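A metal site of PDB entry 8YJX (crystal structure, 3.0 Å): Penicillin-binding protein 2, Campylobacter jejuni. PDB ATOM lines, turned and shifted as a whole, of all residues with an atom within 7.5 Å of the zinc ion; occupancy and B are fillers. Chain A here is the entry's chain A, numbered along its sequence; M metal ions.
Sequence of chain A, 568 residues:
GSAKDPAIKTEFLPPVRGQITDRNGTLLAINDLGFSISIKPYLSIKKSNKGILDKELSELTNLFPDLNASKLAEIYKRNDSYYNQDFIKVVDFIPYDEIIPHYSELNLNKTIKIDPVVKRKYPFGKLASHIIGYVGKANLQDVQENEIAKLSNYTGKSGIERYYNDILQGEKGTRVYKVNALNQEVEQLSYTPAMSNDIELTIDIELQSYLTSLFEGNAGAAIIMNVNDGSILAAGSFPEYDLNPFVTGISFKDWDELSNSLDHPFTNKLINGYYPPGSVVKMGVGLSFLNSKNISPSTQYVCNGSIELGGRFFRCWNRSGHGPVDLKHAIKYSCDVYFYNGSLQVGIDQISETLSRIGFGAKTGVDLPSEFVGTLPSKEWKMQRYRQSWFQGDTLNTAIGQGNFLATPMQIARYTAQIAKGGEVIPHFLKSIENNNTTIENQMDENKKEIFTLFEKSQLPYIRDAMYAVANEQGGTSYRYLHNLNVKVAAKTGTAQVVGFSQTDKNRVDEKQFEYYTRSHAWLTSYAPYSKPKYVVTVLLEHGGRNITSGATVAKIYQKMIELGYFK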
ATOM      1  N   LYS A 282      31.037 -27.375  -9.402  1.00  0.00           N
ATOM      2  CA  LYS A 282      30.743 -26.011  -9.817  1.00  0.00           C
ATOM      3  C   LYS A 282      31.516 -25.009  -8.984  1.00  0.00           C
ATOM      4  O   LYS A 282      32.024 -24.023  -9.524  1.00  0.00           O
ATOM      5  CB  LYS A 282      29.237 -25.783  -9.783  1.00  0.00           C
ATOM      6  CG  LYS A 282      28.537 -26.576 -10.908  1.00  0.00           C
ATOM      7  CD  LYS A 282      27.021 -26.562 -10.819  1.00  0.00           C
ATOM      8  CE  LYS A 282      26.376 -27.302 -11.973  1.00  0.00           C
ATOM      9  NZ  LYS A 282      24.926 -27.484 -11.738  1.00  0.00           N
ATOM     10  N   VAL A 302      21.538 -16.102 -18.830  1.00  0.00           N
ATOM     11  CA  VAL A 302      20.115 -16.429 -18.805  1.00  0.00           C
ATOM     12  C   VAL A 302      19.892 -17.896 -19.167  1.00  0.00           C
ATOM     13  O   VAL A 302      20.326 -18.355 -20.236  1.00  0.00           O
ATOM     14  CB  VAL A 302      19.322 -15.524 -19.739  1.00  0.00           C
ATOM     15  CG1 VAL A 302      17.847 -15.807 -19.540  1.00  0.00           C
ATOM     16  CG2 VAL A 302      19.660 -14.061 -19.473  1.00  0.00           C
ATOM     17  N   CYS A 303      19.184 -18.609 -18.296  1.00  0.00           N
ATOM     18  CA  CYS A 303      18.970 -20.059 -18.437  1.00  0.00           C
ATOM     19  C   CYS A 303      17.532 -20.323 -18.854  1.00  0.00           C
ATOM     20  O   CYS A 303      16.612 -20.267 -18.030  1.00  0.00           O
ATOM     21  CB  CYS A 303      19.289 -20.778 -17.127  1.00  0.00           C
ATOM     22  SG  CYS A 303      18.673 -22.490 -16.963  1.00  0.00           S
ATOM     23  N   ASN A 304      17.324 -20.647 -20.127  1.00  0.00           N
ATOM     24  CA  ASN A 304      15.977 -20.959 -20.570  1.00  0.00           C
ATOM     25  C   ASN A 304      15.721 -22.438 -20.583  1.00  0.00           C
ATOM     26  O   ASN A 304      14.918 -22.915 -21.388  1.00  0.00           O
ATOM     27  CB  ASN A 304      15.685 -20.337 -21.933  1.00  0.00           C
ATOM     28  CG  ASN A 304      15.814 -18.844 -21.907  1.00  0.00           C
ATOM     29  OD1 ASN A 304      16.659 -18.261 -22.593  1.00  0.00           O
ATOM     30  ND2 ASN A 304      14.997 -18.208 -21.060  1.00  0.00           N
ATOM     31  N   GLY A 305      16.381 -23.167 -19.687  1.00  0.00           N
ATOM     32  CA  GLY A 305      16.235 -24.602 -19.619  1.00  0.00           C
ATOM     33  C   GLY A 305      17.096 -25.346 -20.603  1.00  0.00           C
ATOM     34  O   GLY A 305      17.106 -26.588 -20.575  1.00  0.00           O
ATOM     35  N   SER A 306      17.792 -24.635 -21.481  1.00  0.00           N
ATOM     36  CA  SER A 306      18.787 -25.247 -22.344  1.00  0.00           C
ATOM     37  C   SER A 306      19.599 -24.139 -22.980  1.00  0.00           C
ATOM     38  O   SER A 306      19.316 -22.951 -22.789  1.00  0.00           O
ATOM     39  CB  SER A 306      18.147 -26.143 -23.402  1.00  0.00           C
ATOM     40  OG  SER A 306      17.535 -25.401 -24.430  1.00  0.00           O
ATOM     41  N   ARG A 315      20.989 -29.477 -22.095  1.00  0.00           N
ATOM     42  CA  ARG A 315      19.889 -29.129 -21.212  1.00  0.00           C
ATOM     43  C   ARG A 315      20.392 -28.660 -19.841  1.00  0.00           C
ATOM     44  O   ARG A 315      21.509 -28.952 -19.410  1.00  0.00           O
ATOM     45  CB  ARG A 315      18.937 -30.319 -21.020  1.00  0.00           C
ATOM     46  CG  ARG A 315      18.569 -31.077 -22.286  1.00  0.00           C
ATOM     47  CD  ARG A 315      17.143 -30.796 -22.740  1.00  0.00           C
ATOM     48  NE  ARG A 315      16.276 -31.979 -22.727  1.00  0.00           N
ATOM     49  CZ  ARG A 315      15.139 -32.041 -22.045  1.00  0.00           C
ATOM     50  NH1 ARG A 315      14.745 -30.988 -21.338  1.00  0.00           N
ATOM     51  NH2 ARG A 315      14.391 -33.141 -22.065  1.00  0.00           N
ATOM     52  N   CYS A 316      19.559 -27.881 -19.178  1.00  0.00           N
ATOM     53  CA  CYS A 316      19.666 -27.737 -17.735  1.00  0.00           C
ATOM     54  C   CYS A 316      18.818 -28.829 -17.114  1.00  0.00           C
ATOM     55  O   CYS A 316      17.976 -29.440 -17.772  1.00  0.00           O
ATOM     56  CB  CYS A 316      19.230 -26.336 -17.288  1.00  0.00           C
ATOM     57  SG  CYS A 316      19.245 -25.918 -15.542  1.00  0.00           S
ATOM     58  N   TRP A 317      19.065 -29.117 -15.838  1.00  0.00           N
ATOM     59  CA  TRP A 317      18.230 -30.100 -15.178  1.00  0.00           C
ATOM     60  C   TRP A 317      16.837 -29.565 -14.951  1.00  0.00           C
ATOM     61  O   TRP A 317      15.909 -30.354 -14.735  1.00  0.00           O
ATOM     62  CB  TRP A 317      18.846 -30.524 -13.860  1.00  0.00           C
ATOM     63  CG  TRP A 317      18.817 -29.491 -12.756  1.00  0.00           C
ATOM     64  CD1 TRP A 317      19.844 -28.677 -12.378  1.00  0.00           C
ATOM     65  CD2 TRP A 317      17.736 -29.196 -11.858  1.00  0.00           C
ATOM     66  NE1 TRP A 317      19.468 -27.885 -11.318  1.00  0.00           N
ATOM     67  CE2 TRP A 317      18.183 -28.192 -10.978  1.00  0.00           C
ATOM     68  CE3 TRP A 317      16.445 -29.686 -11.727  1.00  0.00           C
ATOM     69  CZ2 TRP A 317      17.379 -27.654  -9.973  1.00  0.00           C
ATOM     70  CZ3 TRP A 317      15.633 -29.153 -10.737  1.00  0.00           C
ATOM     71  CH2 TRP A 317      16.102 -28.137  -9.871  1.00  0.00           C
ATOM     72  N   ASN A 318      16.657 -28.247 -15.000  1.00  0.00           N
ATOM     73  CA  ASN A 318      15.360 -27.605 -14.778  1.00  0.00           C
ATOM     74  C   ASN A 318      14.759 -27.271 -16.147  1.00  0.00           C
ATOM     75  O   ASN A 318      14.997 -26.199 -16.713  1.00  0.00           O
ATOM     76  CB  ASN A 318      15.496 -26.364 -13.907  1.00  0.00           C
ATOM     77  CG  ASN A 318      14.157 -25.701 -13.633  1.00  0.00           C
ATOM     78  OD1 ASN A 318      13.095 -26.289 -13.877  1.00  0.00           O
ATOM     79  ND2 ASN A 318      14.203 -24.493 -13.128  1.00  0.00           N
ATOM     80  N   GLY A 321      13.662 -23.888 -17.073  1.00  0.00           N
ATOM     81  CA  GLY A 321      14.606 -22.787 -17.001  1.00  0.00           C
ATOM     82  C   GLY A 321      14.736 -22.056 -15.673  1.00  0.00           C
ATOM     83  O   GLY A 321      13.769 -21.906 -14.918  1.00  0.00           O
ATOM     84  N   HIS A 322      15.953 -21.599 -15.391  1.00  0.00           N
ATOM     85  CA  HIS A 322      16.270 -20.914 -14.138  1.00  0.00           C
ATOM     86  C   HIS A 322      16.153 -19.409 -14.236  1.00  0.00           C
ATOM     87  O   HIS A 322      16.088 -18.734 -13.211  1.00  0.00           O
ATOM     88  CB  HIS A 322      17.701 -21.197 -13.692  1.00  0.00           C
ATOM     89  CG  HIS A 322      17.866 -22.486 -12.966  1.00  0.00           C
ATOM     90  ND1 HIS A 322      18.338 -23.624 -13.575  1.00  0.00           N
ATOM     91  CD2 HIS A 322      17.611 -22.815 -11.670  1.00  0.00           C
ATOM     92  CE1 HIS A 322      18.376 -24.602 -12.688  1.00  0.00           C
ATOM     93  NE2 HIS A 322      17.943 -24.135 -11.523  1.00  0.00           N
ATOM     94  N   GLY A 323      16.191 -18.876 -15.448  1.00  0.00           N
ATOM     95  CA  GLY A 323      16.133 -17.461 -15.629  1.00  0.00           C
ATOM     96  C   GLY A 323      17.514 -16.885 -15.703  1.00  0.00           C
ATOM     97  O   GLY A 323      18.501 -17.582 -15.973  1.00  0.00           O
ATOM     98  N   VAL A 325      20.738 -15.776 -13.859  1.00  0.00           N
ATOM     99  CA  VAL A 325      21.444 -16.137 -12.634  1.00  0.00           C
ATOM    100  C   VAL A 325      22.855 -15.581 -12.708  1.00  0.00           C
ATOM    101  O   VAL A 325      23.460 -15.527 -13.789  1.00  0.00           O
ATOM    102  CB  VAL A 325      21.502 -17.661 -12.398  1.00  0.00           C
ATOM    103  CG1 VAL A 325      20.147 -18.241 -12.124  1.00  0.00           C
ATOM    104  CG2 VAL A 325      22.133 -18.338 -13.597  1.00  0.00           C
ATOM    105  N   ALA A 330      23.670 -19.456  -9.517  1.00  0.00           N
ATOM    106  CA  ALA A 330      23.871 -20.633 -10.361  1.00  0.00           C
ATOM    107  C   ALA A 330      24.366 -21.806  -9.518  1.00  0.00           C
ATOM    108  O   ALA A 330      24.006 -22.967  -9.785  1.00  0.00           O
ATOM    109  CB  ALA A 330      24.850 -20.305 -11.487  1.00  0.00           C
ATOM    110  N   TYR A 333      21.253 -22.877  -6.983  1.00  0.00           N
ATOM    111  CA  TYR A 333      20.246 -23.693  -7.639  1.00  0.00           C
ATOM    112  C   TYR A 333      20.835 -24.814  -8.471  1.00  0.00           C
ATOM    113  O   TYR A 333      20.079 -25.631  -9.015  1.00  0.00           O
ATOM    114  CB  TYR A 333      19.354 -22.802  -8.510  1.00  0.00           C
ATOM    115  CG  TYR A 333      18.689 -21.673  -7.766  1.00  0.00           C
ATOM    116  CD1 TYR A 333      17.776 -21.919  -6.742  1.00  0.00           C
ATOM    117  CD2 TYR A 333      18.945 -20.356  -8.109  1.00  0.00           C
ATOM    118  CE1 TYR A 333      17.154 -20.870  -6.070  1.00  0.00           C
ATOM    119  CE2 TYR A 333      18.328 -19.309  -7.445  1.00  0.00           C
ATOM    120  CZ  TYR A 333      17.439 -19.570  -6.427  1.00  0.00           C
ATOM    121  OH  TYR A 333      16.837 -18.493  -5.786  1.00  0.00           O
ATOM    122  N   SER A 334      22.158 -24.870  -8.598  1.00  0.00           N
ATOM    123  CA  SER A 334      22.814 -25.865  -9.435  1.00  0.00           C
ATOM    124  C   SER A 334      22.338 -25.742 -10.884  1.00  0.00           C
ATOM    125  O   SER A 334      21.932 -26.724 -11.499  1.00  0.00           O
ATOM    126  CB  SER A 334      22.598 -27.286  -8.878  1.00  0.00           C
ATOM    127  OG  SER A 334      23.572 -28.195  -9.377  1.00  0.00           O
ATOM    128  N   CYS A 335      22.356 -24.520 -11.413  1.00  0.00           N
ATOM    129  CA  CYS A 335      22.043 -24.322 -12.828  1.00  0.00           C
ATOM    130  C   CYS A 335      23.206 -24.820 -13.676  1.00  0.00           C
ATOM    131  O   CYS A 335      24.342 -24.400 -13.484  1.00  0.00           O
ATOM    132  CB  CYS A 335      21.743 -22.847 -13.144  1.00  0.00           C
ATOM    133  SG  CYS A 335      21.602 -22.419 -14.941  1.00  0.00           S
ATOM    134  N   ASP A 336      22.917 -25.733 -14.591  1.00  0.00           N
ATOM    135  CA  ASP A 336      23.941 -26.196 -15.501  1.00  0.00           C
ATOM    136  C   ASP A 336      24.238 -25.134 -16.539  1.00  0.00           C
ATOM    137  O   ASP A 336      25.405 -24.955 -16.942  1.00  0.00           O
ATOM    138  CB  ASP A 336      23.499 -27.519 -16.141  1.00  0.00           C
ATOM    139  CG  ASP A 336      23.163 -28.593 -15.088  1.00  0.00           C
ATOM    140  OD1 ASP A 336      24.058 -28.986 -14.307  1.00  0.00           O
ATOM    141  OD2 ASP A 336      21.993 -29.033 -15.028  1.00  0.00           O
ATOM    142  N   VAL A 337      23.226 -24.366 -16.927  1.00  0.00           N
ATOM    143  CA  VAL A 337      23.349 -23.529 -18.097  1.00  0.00           C
ATOM    144  C   VAL A 337      24.389 -22.434 -17.889  1.00  0.00           C
ATOM    145  O   VAL A 337      25.151 -22.098 -18.815  1.00  0.00           O
ATOM    146  CB  VAL A 337      21.977 -22.953 -18.466  1.00  0.00           C
ATOM    147  CG1 VAL A 337      22.152 -21.880 -19.499  1.00  0.00           C
ATOM    148  CG2 VAL A 337      21.150 -24.068 -19.008  1.00  0.00           C
ATOM    149  N   TYR A 338      24.456 -21.874 -16.675  1.00  0.00           N
ATOM    150  CA  TYR A 338      25.477 -20.886 -16.351  1.00  0.00           C
ATOM    151  C   TYR A 338      26.876 -21.400 -16.654  1.00  0.00           C
ATOM    152  O   TYR A 338      27.685 -20.695 -17.252  1.00  0.00           O
ATOM    153  CB  TYR A 338      25.345 -20.490 -14.876  1.00  0.00           C
ATOM    154  CG  TYR A 338      26.348 -19.454 -14.395  1.00  0.00           C
ATOM    155  CD1 TYR A 338      27.600 -19.829 -13.891  1.00  0.00           C
ATOM    156  CD2 TYR A 338      26.031 -18.107 -14.405  1.00  0.00           C
ATOM    157  CE1 TYR A 338      28.515 -18.887 -13.439  1.00  0.00           C
ATOM    158  CE2 TYR A 338      26.935 -17.170 -13.946  1.00  0.00           C
ATOM    159  CZ  TYR A 338      28.180 -17.574 -13.463  1.00  0.00           C
ATOM    160  OH  TYR A 338      29.072 -16.627 -13.015  1.00  0.00           O
ATOM    161  N   TYR A 340      27.710 -23.948 -18.645  1.00  0.00           N
ATOM    162  CA  TYR A 340      27.816 -24.067 -20.106  1.00  0.00           C
ATOM    163  C   TYR A 340      28.289 -22.768 -20.732  1.00  0.00           C
ATOM    164  O   TYR A 340      29.277 -22.734 -21.489  1.00  0.00           O
ATOM    165  CB  TYR A 340      26.465 -24.424 -20.697  1.00  0.00           C
ATOM    166  CG  TYR A 340      25.914 -25.768 -20.351  1.00  0.00           C
ATOM    167  CD1 TYR A 340      26.708 -26.887 -20.260  1.00  0.00           C
ATOM    168  CD2 TYR A 340      24.565 -25.908 -20.137  1.00  0.00           C
ATOM    169  CE1 TYR A 340      26.158 -28.100 -19.950  1.00  0.00           C
ATOM    170  CE2 TYR A 340      24.022 -27.103 -19.816  1.00  0.00           C
ATOM    171  CZ  TYR A 340      24.804 -28.190 -19.716  1.00  0.00           C
ATOM    172  OH  TYR A 340      24.215 -29.364 -19.395  1.00  0.00           O
HETATM  173 ZN    ZN M   1      19.682 -23.530 -15.073  1.00  0.00          ZN
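The zinc ion is bound by ND1 of His 322, SG of Cys 335, SG of Cys 303 and SG of Cys 316.
SG of Cys 303 sits close to N of Gly 305, 3.6 Å away. The backbone NH (N) of Val 337 lies close to the side-chain sulfur (SG) of Cys 335, 3.2 Å away. O of Ala 330 is in hydrogen-bond range of N of Cys 335 (2.8 Å). The backbone NH (N) of Asp 336 lies close to the side-chain sulfur (SG) of Cys 316 (3.8 Å). The side-chain carboxylate (OD2) of Asp 336 is in hydrogen-bond range of the backbone NH (N) of Trp 317 (3.0 Å). OD1 of Asp 336 lies within salt-bridge range of NZ of Lys 282. N of Cys 316 is in hydrogen-bond range of O of Gly 305 (3.1 Å). The backbone carbonyl oxygen of Gly 323 sits at hydrogen-bond distance from the backbone NH of Cys 303 (2.6 Å).
Asp 336 touches the zinc ion. Within 4 Å of the zinc ion: Cys 303, Cys 316, His 322, Cys 335 and Asp 336. The nearest printed residue that does not touch the zinc ion is Val 337 (4.1 Å).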
